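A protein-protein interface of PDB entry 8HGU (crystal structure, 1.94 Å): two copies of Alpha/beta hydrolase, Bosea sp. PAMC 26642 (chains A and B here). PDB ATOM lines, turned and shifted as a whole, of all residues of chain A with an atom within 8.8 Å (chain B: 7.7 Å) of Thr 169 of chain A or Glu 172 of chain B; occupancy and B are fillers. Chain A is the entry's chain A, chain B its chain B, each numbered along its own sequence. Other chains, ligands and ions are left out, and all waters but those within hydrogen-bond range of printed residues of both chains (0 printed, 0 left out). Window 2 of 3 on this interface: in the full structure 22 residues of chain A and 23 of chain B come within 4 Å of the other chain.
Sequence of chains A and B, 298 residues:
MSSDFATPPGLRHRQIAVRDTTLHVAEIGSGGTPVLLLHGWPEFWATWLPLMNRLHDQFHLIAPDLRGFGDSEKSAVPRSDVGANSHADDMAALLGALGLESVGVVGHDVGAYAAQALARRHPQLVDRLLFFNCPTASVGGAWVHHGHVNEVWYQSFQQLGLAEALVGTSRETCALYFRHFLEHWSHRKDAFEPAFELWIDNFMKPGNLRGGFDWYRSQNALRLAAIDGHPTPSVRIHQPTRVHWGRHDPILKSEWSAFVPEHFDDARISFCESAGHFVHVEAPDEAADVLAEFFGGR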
ATOM      1  N   LEU A 162      23.285 -16.633  18.913  1.00  0.00           N
ATOM      2  CA  LEU A 162      22.863 -17.565  20.004  1.00  0.00           C
ATOM      3  C   LEU A 162      23.054 -16.953  21.407  1.00  0.00           C
ATOM      4  O   LEU A 162      22.208 -17.190  22.251  1.00  0.00           O
ATOM      5  CB  LEU A 162      23.668 -18.862  19.901  1.00  0.00           C
ATOM      6  CG  LEU A 162      23.449 -19.844  21.050  1.00  0.00           C
ATOM      7  CD1 LEU A 162      21.990 -20.296  21.107  1.00  0.00           C
ATOM      8  CD2 LEU A 162      24.378 -21.018  20.896  1.00  0.00           C
ATOM      9  N   ALA A 163      24.134 -16.203  21.641  1.00  0.00           N
ATOM     10  CA  ALA A 163      24.501 -15.602  22.939  1.00  0.00           C
ATOM     11  C   ALA A 163      23.446 -14.586  23.388  1.00  0.00           C
ATOM     12  O   ALA A 163      22.996 -14.700  24.535  1.00  0.00           O
ATOM     13  CB  ALA A 163      25.856 -14.952  22.871  1.00  0.00           C
ATOM     14  N   GLU A 164      23.082 -13.645  22.531  1.00  0.00           N
ATOM     15  CA  GLU A 164      22.034 -12.620  22.796  1.00  0.00           C
ATOM     16  C   GLU A 164      20.680 -13.336  22.974  1.00  0.00           C
ATOM     17  O   GLU A 164      19.951 -12.978  23.892  1.00  0.00           O
ATOM     18  CB  GLU A 164      22.059 -11.568  21.684  1.00  0.00           C
ATOM     19  CG  GLU A 164      21.469 -10.220  22.057  1.00  0.00           C
ATOM     20  CD  GLU A 164      21.508  -9.127  20.978  1.00  0.00           C
ATOM     21  OE1 GLU A 164      22.329  -9.222  19.991  1.00  0.00           O
ATOM     22  OE2 GLU A 164      20.711  -8.147  21.115  1.00  0.00           O
ATOM     23  N   ALA A 165      20.372 -14.373  22.180  1.00  0.00           N
ATOM     24  CA  ALA A 165      19.086 -15.103  22.271  1.00  0.00           C
ATOM     25  C   ALA A 165      18.991 -15.864  23.608  1.00  0.00           C
ATOM     26  O   ALA A 165      17.944 -15.843  24.284  1.00  0.00           O
ATOM     27  CB  ALA A 165      18.953 -16.031  21.091  1.00  0.00           C
ATOM     28  N   LEU A 166      20.048 -16.558  23.992  1.00  0.00           N
ATOM     29  CA  LEU A 166      20.030 -17.499  25.135  1.00  0.00           C
ATOM     30  C   LEU A 166      20.172 -16.685  26.439  1.00  0.00           C
ATOM     31  O   LEU A 166      19.299 -16.818  27.324  1.00  0.00           O
ATOM     32  CB  LEU A 166      21.154 -18.526  24.948  1.00  0.00           C
ATOM     33  CG  LEU A 166      21.337 -19.505  26.092  1.00  0.00           C
ATOM     34  CD1 LEU A 166      20.036 -20.249  26.397  1.00  0.00           C
ATOM     35  CD2 LEU A 166      22.441 -20.506  25.774  1.00  0.00           C
ATOM     36  N   VAL A 167      21.177 -15.814  26.517  1.00  0.00           N
ATOM     37  CA  VAL A 167      21.436 -15.005  27.743  1.00  0.00           C
ATOM     38  C   VAL A 167      20.280 -14.018  27.945  1.00  0.00           C
ATOM     39  O   VAL A 167      19.901 -13.806  29.102  1.00  0.00           O
ATOM     40  CB  VAL A 167      22.808 -14.313  27.672  1.00  0.00           C
ATOM     41  CG1 VAL A 167      23.014 -13.331  28.814  1.00  0.00           C
ATOM     42  CG2 VAL A 167      23.917 -15.355  27.631  1.00  0.00           C
ATOM     43  N   GLY A 168      19.705 -13.516  26.858  1.00  0.00           N
ATOM     44  CA  GLY A 168      18.578 -12.562  26.837  1.00  0.00           C
ATOM     45  C   GLY A 168      17.209 -13.206  26.989  1.00  0.00           C
ATOM     46  O   GLY A 168      16.205 -12.477  26.865  1.00  0.00           O
ATOM     47  N   THR A 169      17.119 -14.505  27.279  1.00  0.00           N
ATOM     48  CA  THR A 169      15.806 -15.184  27.371  1.00  0.00           C
ATOM     49  C   THR A 169      14.950 -14.492  28.430  1.00  0.00           C
ATOM     50  O   THR A 169      13.796 -14.184  28.142  1.00  0.00           O
ATOM     51  CB  THR A 169      15.930 -16.683  27.683  1.00  0.00           C
ATOM     52  OG1 THR A 169      16.433 -17.257  26.485  1.00  0.00           O
ATOM     53  CG2 THR A 169      14.608 -17.323  28.022  1.00  0.00           C
ATOM     54  N   SER A 170      15.504 -14.280  29.620  1.00  0.00           N
ATOM     55  CA  SER A 170      14.754 -13.808  30.802  1.00  0.00           C
ATOM     56  C   SER A 170      15.711 -13.159  31.799  1.00  0.00           C
ATOM     57  O   SER A 170      16.954 -13.361  31.695  1.00  0.00           O
ATOM     58  CB  SER A 170      14.012 -14.972  31.452  1.00  0.00           C
ATOM     59  OG  SER A 170      14.946 -15.923  31.968  1.00  0.00           O
ATOM     60  N   ARG A 171      15.156 -12.485  32.805  1.00  0.00           N
ATOM     61  CA  ARG A 171      15.997 -12.019  33.925  1.00  0.00           C
ATOM     62  C   ARG A 171      16.780 -13.191  34.503  1.00  0.00           C
ATOM     63  O   ARG A 171      17.934 -12.982  34.818  1.00  0.00           O
ATOM     64  CB  ARG A 171      15.223 -11.333  35.038  1.00  0.00           C
ATOM     65  CG  ARG A 171      16.165 -10.441  35.817  1.00  0.00           C
ATOM     66  CD  ARG A 171      15.564  -9.919  37.056  1.00  0.00           C
ATOM     67  NE  ARG A 171      16.610  -9.369  37.897  1.00  0.00           N
ATOM     68  CZ  ARG A 171      16.927  -8.087  37.955  1.00  0.00           C
ATOM     69  NH1 ARG A 171      16.337  -7.212  37.148  1.00  0.00           N
ATOM     70  NH2 ARG A 171      17.873  -7.694  38.787  1.00  0.00           N
ATOM     71  N   GLU A 172      16.144 -14.353  34.710  1.00  0.00           N
ATOM     72  CA  GLU A 172      16.809 -15.550  35.296  1.00  0.00           C
ATOM     73  C   GLU A 172      18.021 -16.002  34.456  1.00  0.00           C
ATOM     74  O   GLU A 172      19.072 -16.341  35.053  1.00  0.00           O
ATOM     75  CB  GLU A 172      15.811 -16.705  35.411  1.00  0.00           C
ATOM     76  CG  GLU A 172      15.696 -17.297  36.802  1.00  0.00           C
ATOM     77  CD  GLU A 172      14.306 -17.858  37.102  1.00  0.00           C
ATOM     78  OE1 GLU A 172      13.314 -17.100  36.959  1.00  0.00           O
ATOM     79  OE2 GLU A 172      14.209 -19.058  37.452  1.00  0.00           O
ATOM     80  N   THR A 173      17.913 -16.088  33.134  1.00  0.00           N
ATOM     81  CA  THR A 173      19.063 -16.508  32.282  1.00  0.00           C
ATOM     82  C   THR A 173      20.151 -15.438  32.350  1.00  0.00           C
ATOM     83  O   THR A 173      21.319 -15.775  32.378  1.00  0.00           O
ATOM     84  CB  THR A 173      18.695 -16.763  30.816  1.00  0.00           C
ATOM     85  OG1 THR A 173      18.104 -15.610  30.209  1.00  0.00           O
ATOM     86  CG2 THR A 173      17.799 -17.975  30.654  1.00  0.00           C
ATOM     87  N   CYS A 174      19.757 -14.172  32.391  1.00  0.00           N
ATOM     88  CA  CYS A 174      20.709 -13.037  32.519  1.00  0.00           C
ATOM     89  C   CYS A 174      21.471 -13.157  33.858  1.00  0.00           C
ATOM     90  O   CYS A 174      22.734 -13.116  33.835  1.00  0.00           O
ATOM     91  CB  CYS A 174      19.959 -11.728  32.327  1.00  0.00           C
ATOM     92  SG  CYS A 174      21.086 -10.323  32.234  1.00  0.00           S
ATOM     93  N   ALA A 175      20.767 -13.460  34.952  1.00  0.00           N
ATOM     94  CA  ALA A 175      21.362 -13.625  36.300  1.00  0.00           C
ATOM     95  C   ALA A 175      22.318 -14.819  36.313  1.00  0.00           C
ATOM     96  O   ALA A 175      23.425 -14.679  36.868  1.00  0.00           O
ATOM     97  CB  ALA A 175      20.303 -13.789  37.353  1.00  0.00           C
ATOM     98  N   PHE A 203      22.334  -5.310  32.691  1.00  0.00           N
ATOM     99  CA  PHE A 203      22.364  -6.223  31.521  1.00  0.00           C
ATOM    100  C   PHE A 203      20.933  -6.564  31.059  1.00  0.00           C
ATOM    101  O   PHE A 203      20.839  -7.135  29.986  1.00  0.00           O
ATOM    102  CB  PHE A 203      23.336  -7.359  31.827  1.00  0.00           C
ATOM    103  CG  PHE A 203      24.782  -6.900  31.777  1.00  0.00           C
ATOM    104  CD1 PHE A 203      25.339  -6.432  30.583  1.00  0.00           C
ATOM    105  CD2 PHE A 203      25.567  -6.859  32.915  1.00  0.00           C
ATOM    106  CE1 PHE A 203      26.661  -5.990  30.523  1.00  0.00           C
ATOM    107  CE2 PHE A 203      26.882  -6.414  32.849  1.00  0.00           C
ATOM    108  CZ  PHE A 203      27.419  -5.944  31.664  1.00  0.00           C
ATOM    109  N   MET A 204      19.871  -6.081  31.717  1.00  0.00           N
ATOM    110  CA  MET A 204      18.469  -6.187  31.207  1.00  0.00           C
ATOM    111  C   MET A 204      18.079  -4.940  30.401  1.00  0.00           C
ATOM    112  O   MET A 204      17.031  -4.966  29.724  1.00  0.00           O
ATOM    113  CB  MET A 204      17.463  -6.400  32.352  1.00  0.00           C
ATOM    114  CG  MET A 204      17.631  -7.740  33.056  1.00  0.00           C
ATOM    115  SD  MET A 204      17.398  -9.137  31.900  1.00  0.00           S
ATOM    116  CE  MET A 204      15.638  -8.965  31.526  1.00  0.00           C
ATOM    117  N   LEU A 209      23.367  -6.272  26.367  1.00  0.00           N
ATOM    118  CA  LEU A 209      24.055  -7.542  25.955  1.00  0.00           C
ATOM    119  C   LEU A 209      24.846  -7.278  24.671  1.00  0.00           C
ATOM    120  O   LEU A 209      26.095  -7.468  24.655  1.00  0.00           O
ATOM    121  CB  LEU A 209      23.050  -8.675  25.735  1.00  0.00           C
ATOM    122  CG  LEU A 209      22.244  -9.126  26.950  1.00  0.00           C
ATOM    123  CD1 LEU A 209      21.431 -10.366  26.615  1.00  0.00           C
ATOM    124  CD2 LEU A 209      23.161  -9.415  28.134  1.00  0.00           C
ATOM    125  N   LEU B 166      21.604 -22.970  32.252  1.00  0.00           N
ATOM    126  CA  LEU B 166      21.154 -22.029  31.206  1.00  0.00           C
ATOM    127  C   LEU B 166      20.410 -22.800  30.122  1.00  0.00           C
ATOM    128  O   LEU B 166      19.227 -22.449  29.811  1.00  0.00           O
ATOM    129  CB  LEU B 166      22.402 -21.313  30.677  1.00  0.00           C
ATOM    130  CG  LEU B 166      22.225 -20.152  29.708  1.00  0.00           C
ATOM    131  CD1 LEU B 166      21.188 -19.154  30.191  1.00  0.00           C
ATOM    132  CD2 LEU B 166      23.568 -19.458  29.515  1.00  0.00           C
ATOM    133  N   VAL B 167      21.053 -23.827  29.560  1.00  0.00           N
ATOM    134  CA  VAL B 167      20.465 -24.581  28.419  1.00  0.00           C
ATOM    135  C   VAL B 167      19.194 -25.249  28.923  1.00  0.00           C
ATOM    136  O   VAL B 167      18.216 -25.300  28.153  1.00  0.00           O
ATOM    137  CB  VAL B 167      21.475 -25.580  27.839  1.00  0.00           C
ATOM    138  CG1 VAL B 167      20.851 -26.509  26.807  1.00  0.00           C
ATOM    139  CG2 VAL B 167      22.638 -24.812  27.256  1.00  0.00           C
ATOM    140  N   THR B 169      17.015 -24.185  31.072  1.00  0.00           N
ATOM    141  CA  THR B 169      16.043 -23.215  31.626  1.00  0.00           C
ATOM    142  C   THR B 169      14.632 -23.630  31.218  1.00  0.00           C
ATOM    143  O   THR B 169      13.775 -23.692  32.097  1.00  0.00           O
ATOM    144  CB  THR B 169      16.338 -21.762  31.235  1.00  0.00           C
ATOM    145  OG1 THR B 169      17.516 -21.371  31.930  1.00  0.00           O
ATOM    146  CG2 THR B 169      15.213 -20.819  31.626  1.00  0.00           C
ATOM    147  N   SER B 170      14.412 -23.939  29.948  1.00  0.00           N
ATOM    148  CA  SER B 170      13.069 -24.246  29.410  1.00  0.00           C
ATOM    149  C   SER B 170      13.211 -25.074  28.149  1.00  0.00           C
ATOM    150  O   SER B 170      14.357 -25.213  27.654  1.00  0.00           O
ATOM    151  CB  SER B 170      12.322 -22.993  29.111  1.00  0.00           C
ATOM    152  OG  SER B 170      12.959 -22.279  28.063  1.00  0.00           O
ATOM    153  N   ARG B 171      12.091 -25.518  27.596  1.00  0.00           N
ATOM    154  CA  ARG B 171      12.095 -26.189  26.272  1.00  0.00           C
ATOM    155  C   ARG B 171      12.660 -25.210  25.243  1.00  0.00           C
ATOM    156  O   ARG B 171      13.397 -25.658  24.365  1.00  0.00           O
ATOM    157  CB  ARG B 171      10.709 -26.676  25.831  1.00  0.00           C
ATOM    158  CG  ARG B 171      10.786 -27.738  24.737  1.00  0.00           C
ATOM    159  CD  ARG B 171       9.471 -28.177  24.125  1.00  0.00           C
ATOM    160  NE  ARG B 171       9.659 -29.037  22.955  1.00  0.00           N
ATOM    161  CZ  ARG B 171       9.871 -30.357  22.974  1.00  0.00           C
ATOM    162  NH1 ARG B 171       9.917 -31.041  24.112  1.00  0.00           N
ATOM    163  NH2 ARG B 171      10.039 -31.000  21.834  1.00  0.00           N
ATOM    164  N   GLU B 172      12.295 -23.930  25.317  1.00  0.00           N
ATOM    165  CA  GLU B 172      12.698 -22.923  24.292  1.00  0.00           C
ATOM    166  C   GLU B 172      14.235 -22.739  24.347  1.00  0.00           C
ATOM    167  O   GLU B 172      14.845 -22.641  23.273  1.00  0.00           O
ATOM    168  CB  GLU B 172      11.952 -21.590  24.489  1.00  0.00           C
ATOM    169  CG  GLU B 172      12.541 -20.806  25.658  1.00  0.00           C
ATOM    170  CD  GLU B 172      11.851 -19.622  26.341  1.00  0.00           C
ATOM    171  OE1 GLU B 172      11.501 -18.635  25.643  1.00  0.00           O
ATOM    172  OE2 GLU B 172      11.780 -19.652  27.620  1.00  0.00           O
ATOM    173  N   THR B 173      14.855 -22.671  25.529  1.00  0.00           N
ATOM    174  CA  THR B 173      16.334 -22.507  25.649  1.00  0.00           C
ATOM    175  C   THR B 173      17.012 -23.780  25.139  1.00  0.00           C
ATOM    176  O   THR B 173      18.031 -23.693  24.498  1.00  0.00           O
ATOM    177  CB  THR B 173      16.845 -22.163  27.054  1.00  0.00           C
ATOM    178  OG1 THR B 173      16.543 -23.151  28.036  1.00  0.00           O
ATOM    179  CG2 THR B 173      16.363 -20.811  27.551  1.00  0.00           C
ATOM    180  N   CYS B 174      16.484 -24.936  25.468  1.00  0.00           N
ATOM    181  CA  CYS B 174      17.011 -26.236  24.996  1.00  0.00           C
ATOM    182  C   CYS B 174      16.942 -26.315  23.456  1.00  0.00           C
ATOM    183  O   CYS B 174      17.958 -26.628  22.816  1.00  0.00           O
ATOM    184  CB  CYS B 174      16.244 -27.339  25.699  1.00  0.00           C
ATOM    185  SG  CYS B 174      16.932 -28.953  25.296  1.00  0.00           S
ATOM    186  N   ALA B 175      15.803 -26.004  22.865  1.00  0.00           N
ATOM    187  CA  ALA B 175      15.600 -26.029  21.406  1.00  0.00           C
ATOM    188  C   ALA B 175      16.595 -25.081  20.716  1.00  0.00           C
ATOM    189  O   ALA B 175      17.176 -25.443  19.693  1.00  0.00           O
ATOM    190  CB  ALA B 175      14.172 -25.665  21.088  1.00  0.00           C
ATOM    191  N   LEU B 176      16.730 -23.868  21.244  1.00  0.00           N
ATOM    192  CA  LEU B 176      17.608 -22.817  20.688  1.00  0.00           C
ATOM    193  C   LEU B 176      19.054 -23.327  20.700  1.00  0.00           C
ATOM    194  O   LEU B 176      19.737 -23.213  19.695  1.00  0.00           O
ATOM    195  CB  LEU B 176      17.418 -21.617  21.613  1.00  0.00           C
ATOM    196  CG  LEU B 176      18.156 -20.350  21.264  1.00  0.00           C
ATOM    197  CD1 LEU B 176      17.653 -19.808  19.924  1.00  0.00           C
ATOM    198  CD2 LEU B 176      17.959 -19.354  22.421  1.00  0.00           C
ATOM    199  N   TYR B 177      19.482 -23.920  21.796  1.00  0.00           N
ATOM    200  CA  TYR B 177      20.877 -24.376  21.949  1.00  0.00           C
ATOM    201  C   TYR B 177      21.159 -25.524  20.971  1.00  0.00           C
ATOM    202  O   TYR B 177      22.141 -25.487  20.210  1.00  0.00           O
ATOM    203  CB  TYR B 177      21.128 -24.835  23.385  1.00  0.00           C
ATOM    204  CG  TYR B 177      22.587 -25.016  23.684  1.00  0.00           C
ATOM    205  CD1 TYR B 177      23.425 -23.916  23.781  1.00  0.00           C
ATOM    206  CD2 TYR B 177      23.154 -26.278  23.790  1.00  0.00           C
ATOM    207  CE1 TYR B 177      24.776 -24.072  24.082  1.00  0.00           C
ATOM    208  CE2 TYR B 177      24.508 -26.442  24.081  1.00  0.00           C
ATOM    209  CZ  TYR B 177      25.323 -25.329  24.209  1.00  0.00           C
ATOM    210  OH  TYR B 177      26.666 -25.466  24.453  1.00  0.00           O
ATOM    211  N   PHE B 178      20.331 -26.560  20.999  1.00  0.00           N
ATOM    212  CA  PHE B 178      20.585 -27.778  20.189  1.00  0.00           C
ATOM    213  C   PHE B 178      20.375 -27.475  18.708  1.00  0.00           C
ATOM    214  O   PHE B 178      21.156 -28.031  17.935  1.00  0.00           O
ATOM    215  CB  PHE B 178      19.831 -28.989  20.732  1.00  0.00           C
ATOM    216  CG  PHE B 178      20.491 -29.528  21.973  1.00  0.00           C
ATOM    217  CD1 PHE B 178      21.563 -30.399  21.890  1.00  0.00           C
ATOM    218  CD2 PHE B 178      20.085 -29.114  23.227  1.00  0.00           C
ATOM    219  CE1 PHE B 178      22.158 -30.905  23.037  1.00  0.00           C
ATOM    220  CE2 PHE B 178      20.699 -29.582  24.375  1.00  0.00           C
ATOM    221  CZ  PHE B 178      21.729 -30.496  24.281  1.00  0.00           C
ATOM    222  N   PHE B 196      13.485 -33.284  14.804  1.00  0.00           N
ATOM    223  CA  PHE B 196      13.892 -32.167  15.708  1.00  0.00           C
ATOM    224  C   PHE B 196      13.115 -32.278  17.032  1.00  0.00           C
ATOM    225  O   PHE B 196      13.740 -32.192  18.115  1.00  0.00           O
ATOM    226  CB  PHE B 196      13.729 -30.788  15.068  1.00  0.00           C
ATOM    227  CG  PHE B 196      14.266 -29.695  15.961  1.00  0.00           C
ATOM    228  CD1 PHE B 196      15.632 -29.595  16.200  1.00  0.00           C
ATOM    229  CD2 PHE B 196      13.411 -28.849  16.651  1.00  0.00           C
ATOM    230  CE1 PHE B 196      16.142 -28.626  17.055  1.00  0.00           C
ATOM    231  CE2 PHE B 196      13.925 -27.893  17.521  1.00  0.00           C
ATOM    232  CZ  PHE B 196      15.286 -27.774  17.706  1.00  0.00           C
ATOM    233  N   ILE B 200      14.751 -32.701  20.871  1.00  0.00           N
ATOM    234  CA  ILE B 200      14.524 -31.822  22.053  1.00  0.00           C
ATOM    235  C   ILE B 200      13.912 -32.653  23.197  1.00  0.00           C
ATOM    236  O   ILE B 200      14.342 -32.494  24.371  1.00  0.00           O
ATOM    237  CB  ILE B 200      13.687 -30.595  21.638  1.00  0.00           C
ATOM    238  CG1 ILE B 200      14.348 -29.884  20.458  1.00  0.00           C
ATOM    239  CG2 ILE B 200      13.459 -29.657  22.828  1.00  0.00           C
ATOM    240  CD1 ILE B 200      15.828 -29.655  20.634  1.00  0.00           C
ATOM    241  N   MET B 204      15.515 -32.873  26.982  1.00  0.00           N
ATOM    242  CA  MET B 204      14.633 -32.398  28.082  1.00  0.00           C
ATOM    243  C   MET B 204      14.488 -33.509  29.120  1.00  0.00           C
ATOM    244  O   MET B 204      14.069 -33.206  30.233  1.00  0.00           O
ATOM    245  CB  MET B 204      13.238 -32.013  27.569  1.00  0.00           C
ATOM    246  CG  MET B 204      13.219 -30.718  26.786  1.00  0.00           C
ATOM    247  SD  MET B 204      13.827 -29.306  27.734  1.00  0.00           S
ATOM    248  CE  MET B 204      12.398 -28.987  28.784  1.00  0.00           C
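The backbone carbonyl oxygen of Leu 166 of chain A sits at hydrogen-bond distance from the side-chain hydroxyl of Thr 173 of chain A. OG1 of Thr 173 of chain A sits at hydrogen-bond distance from O of Val 167 of chain A, at 2.8 Å. O of Leu 166 of chain B lies within hydrogen-bond range of OG1 of Thr 173 of chain B (3.3 Å). The backbone carbonyl oxygen (O) of Val 167 of chain B sits at hydrogen-bond distance from the side-chain hydroxyl (OG1) of Thr 173 of chain B. N of Thr 169 of chain B lies within hydrogen-bond range of OG1 of Thr 173 of chain B. The side-chain hydroxyl (OG) of Ser 170 of chain B lies close to the side-chain carboxylate (OE2) of Glu 172 of chain B.
Leu 166 of chain A touches its own counterpart, Leu 166 of chain B. Leu 166 of chain A touches Thr 173 of chain B, and with the chains exchanged Thr 173 of chain A touches Leu 166 of chain B. Thr 169 of chain A touches Glu 172 of chain B, but with the chains exchanged Glu 172 of chain A does not touch Thr 169 of chain B (5.6 Å). Thr 169 of chain A touches Thr 173 of chain B, and with the chains exchanged Thr 173 of chain A touches Thr 169 of chain B. Positions printed for both chains: 166, 167, 169, 170, 171, 172, 173, 174, 175 and 204.
Printed residues of chain B within 4 Å of Leu 162 of chain A: Leu 176 (3.8 Å). Printed residues of chain B within 4 Å of Ala 165 of chain A: Leu 176. Of the printed residues of chain B, Leu 166 of chain A touches Leu 166, Thr 173 and Leu 176. No residue of chain B comes within 4 Å of Gly 168 of chain A. Thr 169 of chain A touches two residues of chain B. Printed residues of chain B within 4 Å of Thr 173 of chain A: Leu 166 and Thr 169. Printed residues of chain A within 4 Å of Leu 166 of chain B: Leu 166 and Thr 173. Arg 171 of chain B touches none of the printed residues of chain A. Glu 172 of chain B touches just one residue of chain A: Thr 169. Of chain A, only Leu 166 (3.8 Å) and Thr 169 (3.7 Å) come within 4 Å of Thr 173 of chain B. Phe 178 of chain B touches none of the printed residues of chain A. The nearest residue of chain A that does not touch Glu 172 of chain B is Ser 170 of chain A (6.4 Å). The nearest printed residue of chain B that does not touch Thr 173 of chain A is Thr 173 of chain B (4.4 Å).
Among the printed residues, merely in contact across the chains: Leu 162 of chain A with Leu 176 of chain B (3.8 Å), Ala 165 of chain A with Leu 176 of chain B (3.7 Å), Leu 166 of chain A with Leu 166 of chain B (3.8 Å), Leu 166 of chain A with Thr 173 of chain B (3.8 Å), Leu 166 of chain A with Leu 176 of chain B (3.8 Å), Thr 169 of chain A with Glu 172 of chain B (3.7 Å), Thr 169 of chain A with Thr 173 of chain B (3.7 Å), Thr 173 of chain A with Leu 166 of chain B (3.5 Å) and Thr 173 of chain A with Thr 169 of chain B (3.6 Å).
Of the 15 printed residues of chain B, 5 touch a printed residue of chain A. Printed residues of chain B that touch a printed residue of chain A: Leu 166, Thr 169, Glu 172, Thr 173 and Leu 176. Hydrophobic or aromatic side chains of chain B that line the printed part of chain A: Leu 166 and Leu 176.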
